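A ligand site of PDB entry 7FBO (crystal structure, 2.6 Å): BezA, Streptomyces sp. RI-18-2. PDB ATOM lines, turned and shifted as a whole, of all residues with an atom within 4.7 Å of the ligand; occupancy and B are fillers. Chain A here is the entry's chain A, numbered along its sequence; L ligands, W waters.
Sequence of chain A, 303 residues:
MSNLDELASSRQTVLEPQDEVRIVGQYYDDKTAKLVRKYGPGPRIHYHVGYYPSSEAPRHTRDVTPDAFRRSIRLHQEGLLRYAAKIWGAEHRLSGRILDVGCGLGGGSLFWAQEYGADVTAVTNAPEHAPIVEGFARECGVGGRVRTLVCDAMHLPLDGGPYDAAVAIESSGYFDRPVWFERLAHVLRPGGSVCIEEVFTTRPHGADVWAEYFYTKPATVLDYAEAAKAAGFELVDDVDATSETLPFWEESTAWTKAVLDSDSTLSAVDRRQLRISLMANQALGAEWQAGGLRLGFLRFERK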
ATOM      1  N   VAL A  24     -18.861  15.024  -6.091  1.00  0.00           N
ATOM      2  CA  VAL A  24     -18.524  14.320  -7.324  1.00  0.00           C
ATOM      3  C   VAL A  24     -19.243  12.974  -7.398  1.00  0.00           C
ATOM      4  O   VAL A  24     -19.574  12.493  -8.499  1.00  0.00           O
ATOM      5  CB  VAL A  24     -16.993  14.182  -7.495  1.00  0.00           C
ATOM      6  CG1 VAL A  24     -16.250  14.715  -6.287  1.00  0.00           C
ATOM      7  CG2 VAL A  24     -16.572  12.737  -7.814  1.00  0.00           C
ATOM      8  N   TYR A  28     -21.369  11.846 -10.634  1.00  0.00           N
ATOM      9  CA  TYR A  28     -21.296  10.577 -11.350  1.00  0.00           C
ATOM     10  C   TYR A  28     -22.651   9.898 -11.456  1.00  0.00           C
ATOM     11  O   TYR A  28     -22.958   9.271 -12.473  1.00  0.00           O
ATOM     12  CB  TYR A  28     -20.245   9.660 -10.689  1.00  0.00           C
ATOM     13  CG  TYR A  28     -18.916   9.823 -11.379  1.00  0.00           C
ATOM     14  CD1 TYR A  28     -18.696   9.229 -12.612  1.00  0.00           C
ATOM     15  CD2 TYR A  28     -17.914  10.639 -10.855  1.00  0.00           C
ATOM     16  CE1 TYR A  28     -17.517   9.397 -13.291  1.00  0.00           C
ATOM     17  CE2 TYR A  28     -16.728  10.810 -11.526  1.00  0.00           C
ATOM     18  CZ  TYR A  28     -16.536  10.186 -12.752  1.00  0.00           C
ATOM     19  OH  TYR A  28     -15.373  10.337 -13.466  1.00  0.00           O
ATOM     20  N   ILE A  45     -19.409  -1.727 -19.954  1.00  0.00           N
ATOM     21  CA  ILE A  45     -19.462  -0.297 -20.263  1.00  0.00           C
ATOM     22  C   ILE A  45     -18.248   0.361 -19.629  1.00  0.00           C
ATOM     23  O   ILE A  45     -18.069   0.315 -18.391  1.00  0.00           O
ATOM     24  CB  ILE A  45     -20.773   0.346 -19.780  1.00  0.00           C
ATOM     25  CG1 ILE A  45     -21.982  -0.451 -20.274  1.00  0.00           C
ATOM     26  CG2 ILE A  45     -20.868   1.775 -20.273  1.00  0.00           C
ATOM     27  CD1 ILE A  45     -23.304   0.114 -19.810  1.00  0.00           C
ATOM     28  N   HIS A  46     -17.418   0.978 -20.460  1.00  0.00           N
ATOM     29  CA  HIS A  46     -16.158   1.576 -20.084  1.00  0.00           C
ATOM     30  C   HIS A  46     -16.274   3.096 -20.044  1.00  0.00           C
ATOM     31  O   HIS A  46     -16.959   3.691 -20.889  1.00  0.00           O
ATOM     32  CB  HIS A  46     -15.066   1.168 -21.048  1.00  0.00           C
ATOM     33  CG  HIS A  46     -14.858  -0.314 -21.116  1.00  0.00           C
ATOM     34  ND1 HIS A  46     -14.369  -1.046 -20.059  1.00  0.00           N
ATOM     35  CD2 HIS A  46     -15.097  -1.201 -22.109  1.00  0.00           C
ATOM     36  CE1 HIS A  46     -14.292  -2.318 -20.399  1.00  0.00           C
ATOM     37  NE2 HIS A  46     -14.729  -2.439 -21.637  1.00  0.00           N
ATOM     38  N   TYR A  47     -15.609   3.720 -19.060  1.00  0.00           N
ATOM     39  CA  TYR A  47     -15.552   5.162 -18.942  1.00  0.00           C
ATOM     40  C   TYR A  47     -14.110   5.590 -18.733  1.00  0.00           C
ATOM     41  O   TYR A  47     -13.714   6.099 -17.673  1.00  0.00           O
ATOM     42  CB  TYR A  47     -16.443   5.653 -17.799  1.00  0.00           C
ATOM     43  CG  TYR A  47     -16.684   7.128 -17.866  1.00  0.00           C
ATOM     44  CD1 TYR A  47     -16.943   7.748 -19.084  1.00  0.00           C
ATOM     45  CD2 TYR A  47     -16.656   7.923 -16.720  1.00  0.00           C
ATOM     46  CE1 TYR A  47     -17.157   9.094 -19.160  1.00  0.00           C
ATOM     47  CE2 TYR A  47     -16.870   9.270 -16.796  1.00  0.00           C
ATOM     48  CZ  TYR A  47     -17.120   9.861 -18.012  1.00  0.00           C
ATOM     49  OH  TYR A  47     -17.340  11.205 -18.110  1.00  0.00           O
ATOM     50  N   HIS A  48     -13.289   5.334 -19.751  1.00  0.00           N
ATOM     51  CA  HIS A  48     -11.903   5.806 -19.800  1.00  0.00           C
ATOM     52  C   HIS A  48     -11.578   6.098 -21.261  1.00  0.00           C
ATOM     53  O   HIS A  48     -12.374   5.835 -22.162  1.00  0.00           O
ATOM     54  CB  HIS A  48     -10.910   4.795 -19.194  1.00  0.00           C
ATOM     55  CG  HIS A  48     -11.105   3.378 -19.656  1.00  0.00           C
ATOM     56  ND1 HIS A  48     -11.886   2.475 -18.983  1.00  0.00           N
ATOM     57  CD2 HIS A  48     -10.607   2.722 -20.731  1.00  0.00           C
ATOM     58  CE1 HIS A  48     -11.868   1.308 -19.612  1.00  0.00           C
ATOM     59  NE2 HIS A  48     -11.101   1.432 -20.681  1.00  0.00           N
ATOM     60  N   ASP A 100     -10.913  -3.235  -7.617  1.00  0.00           N
ATOM     61  CA  ASP A 100     -11.105  -2.381  -8.778  1.00  0.00           C
ATOM     62  C   ASP A 100     -11.670  -1.077  -8.238  1.00  0.00           C
ATOM     63  O   ASP A 100     -12.878  -0.979  -7.987  1.00  0.00           O
ATOM     64  CB  ASP A 100     -12.010  -3.042  -9.808  1.00  0.00           C
ATOM     65  CG  ASP A 100     -12.281  -2.151 -10.994  1.00  0.00           C
ATOM     66  OD1 ASP A 100     -11.450  -1.279 -11.297  1.00  0.00           O
ATOM     67  OD2 ASP A 100     -13.335  -2.338 -11.642  1.00  0.00           O
ATOM     68  N   GLY A 102     -12.783   2.744  -8.100  1.00  0.00           N
ATOM     69  CA  GLY A 102     -13.400   3.662  -9.033  1.00  0.00           C
ATOM     70  C   GLY A 102     -13.830   2.892 -10.254  1.00  0.00           C
ATOM     71  O   GLY A 102     -13.172   2.962 -11.288  1.00  0.00           O
ATOM     72  N   CYS A 103     -14.929   2.147 -10.139  1.00  0.00           N
ATOM     73  CA  CYS A 103     -15.222   1.077 -11.076  1.00  0.00           C
ATOM     74  C   CYS A 103     -16.159   1.495 -12.204  1.00  0.00           C
ATOM     75  O   CYS A 103     -16.404   0.693 -13.107  1.00  0.00           O
ATOM     76  CB  CYS A 103     -15.797  -0.124 -10.323  1.00  0.00           C
ATOM     77  SG  CYS A 103     -17.468   0.086  -9.642  1.00  0.00           S
ATOM     78  N   GLY A 104     -16.639   2.739 -12.197  1.00  0.00           N
ATOM     79  CA  GLY A 104     -17.548   3.158 -13.253  1.00  0.00           C
ATOM     80  C   GLY A 104     -18.816   2.321 -13.288  1.00  0.00           C
ATOM     81  O   GLY A 104     -19.488   2.109 -12.262  1.00  0.00           O
ATOM     82  N   VAL A 123     -15.229  -0.839  -6.363  1.00  0.00           N
ATOM     83  CA  VAL A 123     -15.476   0.248  -5.425  1.00  0.00           C
ATOM     84  C   VAL A 123     -15.914   1.481  -6.209  1.00  0.00           C
ATOM     85  O   VAL A 123     -15.392   1.747  -7.297  1.00  0.00           O
ATOM     86  CB  VAL A 123     -14.200   0.545  -4.599  1.00  0.00           C
ATOM     87  CG1 VAL A 123     -14.394   1.792  -3.750  1.00  0.00           C
ATOM     88  CG2 VAL A 123     -13.810  -0.680  -3.759  1.00  0.00           C
ATOM     89  N   THR A 124     -16.902   2.208  -5.672  1.00  0.00           N
ATOM     90  CA  THR A 124     -17.330   3.474  -6.267  1.00  0.00           C
ATOM     91  C   THR A 124     -18.042   4.313  -5.210  1.00  0.00           C
ATOM     92  O   THR A 124     -18.510   3.788  -4.197  1.00  0.00           O
ATOM     93  CB  THR A 124     -18.254   3.273  -7.463  1.00  0.00           C
ATOM     94  OG1 THR A 124     -18.825   4.535  -7.827  1.00  0.00           O
ATOM     95  CG2 THR A 124     -19.378   2.341  -7.108  1.00  0.00           C
ATOM     96  N   ASN A 125     -18.107   5.616  -5.465  1.00  0.00           N
ATOM     97  CA  ASN A 125     -18.867   6.544  -4.632  1.00  0.00           C
ATOM     98  C   ASN A 125     -20.151   7.008  -5.303  1.00  0.00           C
ATOM     99  O   ASN A 125     -20.785   7.951  -4.828  1.00  0.00           O
ATOM    100  CB  ASN A 125     -17.990   7.756  -4.239  1.00  0.00           C
ATOM    101  CG  ASN A 125     -17.692   8.703  -5.420  1.00  0.00           C
ATOM    102  OD1 ASN A 125     -17.926   8.387  -6.596  1.00  0.00           O
ATOM    103  ND2 ASN A 125     -17.147   9.889  -5.104  1.00  0.00           N
ATOM    104  N   ALA A 126     -20.525   6.387  -6.428  1.00  0.00           N
ATOM    105  CA  ALA A 126     -21.780   6.691  -7.113  1.00  0.00           C
ATOM    106  C   ALA A 126     -22.748   5.553  -6.846  1.00  0.00           C
ATOM    107  O   ALA A 126     -22.628   4.482  -7.462  1.00  0.00           O
ATOM    108  CB  ALA A 126     -21.561   6.873  -8.622  1.00  0.00           C
ATOM    109  N   CYS A 151     -19.023   3.566  -1.256  1.00  0.00           N
ATOM    110  CA  CYS A 151     -17.755   3.708  -0.552  1.00  0.00           C
ATOM    111  C   CYS A 151     -17.102   5.023  -0.939  1.00  0.00           C
ATOM    112  O   CYS A 151     -17.339   5.573  -2.012  1.00  0.00           O
ATOM    113  CB  CYS A 151     -16.846   2.552  -0.941  1.00  0.00           C
ATOM    114  SG  CYS A 151     -15.680   2.021   0.238  1.00  0.00           S
ATOM    115  N   ASP A 152     -16.242   5.505  -0.059  1.00  0.00           N
ATOM    116  CA  ASP A 152     -15.152   6.382  -0.462  1.00  0.00           C
ATOM    117  C   ASP A 152     -13.899   5.509  -0.520  1.00  0.00           C
ATOM    118  O   ASP A 152     -13.672   4.675   0.365  1.00  0.00           O
ATOM    119  CB  ASP A 152     -14.981   7.552   0.511  1.00  0.00           C
ATOM    120  CG  ASP A 152     -13.846   8.475   0.122  1.00  0.00           C
ATOM    121  OD1 ASP A 152     -13.745   8.854  -1.065  1.00  0.00           O
ATOM    122  OD2 ASP A 152     -13.047   8.823   1.020  1.00  0.00           O
ATOM    123  N   ALA A 153     -13.117   5.658  -1.597  1.00  0.00           N
ATOM    124  CA  ALA A 153     -12.034   4.720  -1.884  1.00  0.00           C
ATOM    125  C   ALA A 153     -11.044   4.625  -0.732  1.00  0.00           C
ATOM    126  O   ALA A 153     -10.427   3.571  -0.523  1.00  0.00           O
ATOM    127  CB  ALA A 153     -11.306   5.138  -3.156  1.00  0.00           C
ATOM    128  N   MET A 154     -10.880   5.709   0.011  1.00  0.00           N
ATOM    129  CA  MET A 154      -9.804   5.885   0.964  1.00  0.00           C
ATOM    130  C   MET A 154     -10.332   5.948   2.393  1.00  0.00           C
ATOM    131  O   MET A 154      -9.816   6.696   3.234  1.00  0.00           O
ATOM    132  CB  MET A 154      -9.014   7.141   0.611  1.00  0.00           C
ATOM    133  CG  MET A 154      -9.910   8.224  -0.024  1.00  0.00           C
ATOM    134  SD  MET A 154      -9.048   9.353  -1.142  1.00  0.00           S
ATOM    135  CE  MET A 154     -10.327  10.556  -1.535  1.00  0.00           C
ATOM    136  N   ILE A 169      -8.443   2.539 -12.973  1.00  0.00           N
ATOM    137  CA  ILE A 169      -8.383   2.959 -14.360  1.00  0.00           C
ATOM    138  C   ILE A 169      -9.071   4.323 -14.412  1.00  0.00           C
ATOM    139  O   ILE A 169     -10.309   4.411 -14.409  1.00  0.00           O
ATOM    140  CB  ILE A 169      -9.067   1.953 -15.295  1.00  0.00           C
ATOM    141  CG1 ILE A 169      -8.318   0.612 -15.376  1.00  0.00           C
ATOM    142  CG2 ILE A 169      -9.171   2.540 -16.699  1.00  0.00           C
ATOM    143  CD1 ILE A 169      -6.832   0.689 -15.592  1.00  0.00           C
ATOM    144  N   GLU A 170      -8.278   5.396 -14.426  1.00  0.00           N
ATOM    145  CA  GLU A 170      -8.746   6.772 -14.601  1.00  0.00           C
ATOM    146  C   GLU A 170      -9.634   7.254 -13.458  1.00  0.00           C
ATOM    147  O   GLU A 170     -10.433   8.179 -13.624  1.00  0.00           O
ATOM    148  CB  GLU A 170      -9.479   6.952 -15.934  1.00  0.00           C
ATOM    149  CG  GLU A 170      -8.766   7.916 -16.859  1.00  0.00           C
ATOM    150  CD  GLU A 170      -9.382   7.942 -18.233  1.00  0.00           C
ATOM    151  OE1 GLU A 170     -10.478   8.542 -18.380  1.00  0.00           O
ATOM    152  OE2 GLU A 170      -8.814   7.337 -19.153  1.00  0.00           O
ATOM    153  N   SER A 171      -9.488   6.638 -12.292  1.00  0.00           N
ATOM    154  CA  SER A 171     -10.182   7.068 -11.086  1.00  0.00           C
ATOM    155  C   SER A 171      -9.278   7.709 -10.033  1.00  0.00           C
ATOM    156  O   SER A 171      -9.778   8.499  -9.225  1.00  0.00           O
ATOM    157  CB  SER A 171     -10.891   5.872 -10.450  1.00  0.00           C
ATOM    158  OG  SER A 171      -9.929   4.938 -10.010  1.00  0.00           O
ATOM    159  N   TYR A 174      -9.329  11.358  -8.406  1.00  0.00           N
ATOM    160  CA  TYR A 174     -10.262  11.820  -7.384  1.00  0.00           C
ATOM    161  C   TYR A 174      -9.775  11.523  -5.981  1.00  0.00           C
ATOM    162  O   TYR A 174     -10.508  11.783  -5.017  1.00  0.00           O
ATOM    163  CB  TYR A 174     -11.643  11.180  -7.591  1.00  0.00           C
ATOM    164  CG  TYR A 174     -12.283  11.580  -8.888  1.00  0.00           C
ATOM    165  CD1 TYR A 174     -12.835  12.847  -9.032  1.00  0.00           C
ATOM    166  CD2 TYR A 174     -12.319  10.711  -9.975  1.00  0.00           C
ATOM    167  CE1 TYR A 174     -13.382  13.230 -10.213  1.00  0.00           C
ATOM    168  CE2 TYR A 174     -12.876  11.080 -11.155  1.00  0.00           C
ATOM    169  CZ  TYR A 174     -13.405  12.345 -11.278  1.00  0.00           C
ATOM    170  OH  TYR A 174     -13.995  12.745 -12.453  1.00  0.00           O
ATOM    171  N   PHE A 175      -8.598  10.949  -5.833  1.00  0.00           N
ATOM    172  CA  PHE A 175      -8.165  10.409  -4.550  1.00  0.00           C
ATOM    173  C   PHE A 175      -7.094  11.283  -3.927  1.00  0.00           C
ATOM    174  O   PHE A 175      -6.400  12.041  -4.625  1.00  0.00           O
ATOM    175  CB  PHE A 175      -7.634   8.985  -4.698  1.00  0.00           C
ATOM    176  CG  PHE A 175      -8.618   8.024  -5.301  1.00  0.00           C
ATOM    177  CD1 PHE A 175      -9.978   8.304  -5.308  1.00  0.00           C
ATOM    178  CD2 PHE A 175      -8.187   6.835  -5.856  1.00  0.00           C
ATOM    179  CE1 PHE A 175     -10.878   7.425  -5.849  1.00  0.00           C
ATOM    180  CE2 PHE A 175      -9.077   5.947  -6.418  1.00  0.00           C
ATOM    181  CZ  PHE A 175     -10.429   6.251  -6.411  1.00  0.00           C
HETATM  182  N1  LIG L   1     -12.722   2.073 -13.977  1.00  0.00           N
HETATM  183  C1  LIG L   1     -13.783   2.883 -14.591  1.00  0.00           C
HETATM  184  C2  LIG L   1     -13.567   4.327 -14.158  1.00  0.00           C
HETATM  185  C3  LIG L   1     -14.754   5.273 -14.114  1.00  0.00           C
HETATM  186  S1  LIG L   1     -14.137   6.985 -14.085  1.00  0.00           S
HETATM  187  C4  LIG L   1     -13.786   2.741 -16.122  1.00  0.00           C
HETATM  188  O1  LIG L   1     -14.771   2.314 -16.766  1.00  0.00           O
HETATM  189  O2  LIG L   1     -12.762   3.041 -16.731  1.00  0.00           O
HETATM  190  C5  LIG L   1     -14.219   7.363 -12.317  1.00  0.00           C
HETATM  191  C6  LIG L   1     -14.666   6.287 -11.333  1.00  0.00           C
HETATM  192  O3  LIG L   1     -14.104   6.596 -10.064  1.00  0.00           O
HETATM  193  C7  LIG L   1     -16.172   6.276 -11.148  1.00  0.00           C
HETATM  194  O4  LIG L   1     -16.557   4.961 -10.783  1.00  0.00           O
HETATM  195  C8  LIG L   1     -16.380   7.136  -9.932  1.00  0.00           C
HETATM  196  O5  LIG L   1     -17.597   6.785  -9.311  1.00  0.00           O
HETATM  197  C9  LIG L   1     -15.168   6.707  -9.137  1.00  0.00           C
HETATM  198  N2  LIG L   1     -14.863   7.591  -7.981  1.00  0.00           N
HETATM  199  C10 LIG L   1     -14.789   8.959  -7.994  1.00  0.00           C
HETATM  200  N3  LIG L   1     -14.510   9.388  -6.729  1.00  0.00           N
HETATM  201  C11 LIG L   1     -14.425   8.305  -5.937  1.00  0.00           C
HETATM  202  C12 LIG L   1     -14.169   8.195  -4.582  1.00  0.00           C
HETATM  203  N4  LIG L   1     -13.965   9.319  -3.918  1.00  0.00           N
HETATM  204  N5  LIG L   1     -14.123   6.987  -3.963  1.00  0.00           N
HETATM  205  C13 LIG L   1     -14.355   5.859  -4.727  1.00  0.00           C
HETATM  206  N6  LIG L   1     -14.616   5.958  -6.075  1.00  0.00           N
HETATM  207  C14 LIG L   1     -14.654   7.169  -6.686  1.00  0.00           C
HETATM  208  O   HOH W   1     -19.308   4.252 -10.744  1.00  0.00           O
HETATM  209  O   HOH W   2     -14.633  11.748  -4.993  1.00  0.00           O
HETATM  210  O   HOH W   3     -11.017   1.222 -12.037  1.00  0.00           O
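Residues that only touch the ligand: His 46 (3.7 Å), Glu 170 (3.9 Å), Ser 171 (3.3 Å), Tyr 174 (3.5 Å) and Phe 175 (3.6 Å). Hydrophobic or aromatic side chains that line the ligand: Tyr 28, Tyr 47, His 48, Ala 153, Ile 169, Tyr 174 and Phe 175. Of the 23 residues printed, 16 come within 4 Å of the ligand.
A ring nitrogen (ND1) of His 48 is in hydrogen-bond range of an oxygen (O2) of the ligand. The backbone NH of Gly 104 is in hydrogen-bond range of an oxygen (O4) of the ligand (2.6 Å). N of Tyr 47 sits at hydrogen-bond distance from O1 of the ligand (2.8 Å). A nitrogen (N1) of the ligand is in hydrogen-bond range of the backbone carbonyl oxygen of Gly 102, at 2.9 Å. The backbone NH of Ala 153 sits at hydrogen-bond distance from a nitrogen (N5) of the ligand. The side-chain carboxylate (OD1) of Asp 152 sits at hydrogen-bond distance from a nitrogen (N4) of the ligand (2.9 Å). An oxygen (O5) of the ligand is in hydrogen-bond range of the side-chain hydroxyl (OG1) of Thr 124, at 3.0 Å. N3 of the ligand is in hydrogen-bond range of ND2 of Asn 125, at 3.1 Å. The backbone carbonyl oxygen (O) of Ile 169 lies close to a nitrogen (N1) of the ligand, 3.4 Å away. An oxygen (O4) of the ligand is in hydrogen-bond range of the backbone NH of Cys 103, 3.3 Å away. S1 of the ligand sits close to OH of Tyr 28 (3.6 Å).
N of Gly 102 lies within hydrogen-bond range of O of Val 123, 2.9 Å away. The backbone carbonyl oxygen (O) of Thr 124 sits at hydrogen-bond distance from the backbone NH (N) of Cys 151 (3.0 Å). The side-chain hydroxyl of Thr 124 is in hydrogen-bond range of the backbone NH of Ala 126 (2.9 Å). The backbone NH (N) of Cys 103 lies within hydrogen-bond range of the backbone carbonyl oxygen (O) of Val 123 (2.9 Å). The side-chain hydroxyl (OH) of Tyr 28 sits at hydrogen-bond distance from the side-chain hydroxyl (OH) of Tyr 174.
Water W3 lies within hydrogen-bond range of the side-chain carboxylate of Asp 100 (2.6 Å), a nitrogen (N1) of the ligand (2.7 Å), the backbone carbonyl oxygen of Gly 102 (2.9 Å) and the backbone NH of Ile 169 (3.0 Å). Water W2 bridges a nitrogen (N4) of the ligand (2.7 Å) and the side-chain amide nitrogen (ND2) of Asn 125 (3.1 Å). Water W1 lies within hydrogen-bond range of O of Gly 104 (2.6 Å), O4 of the ligand (2.8 Å) and OG1 of Thr 124 (3.0 Å).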
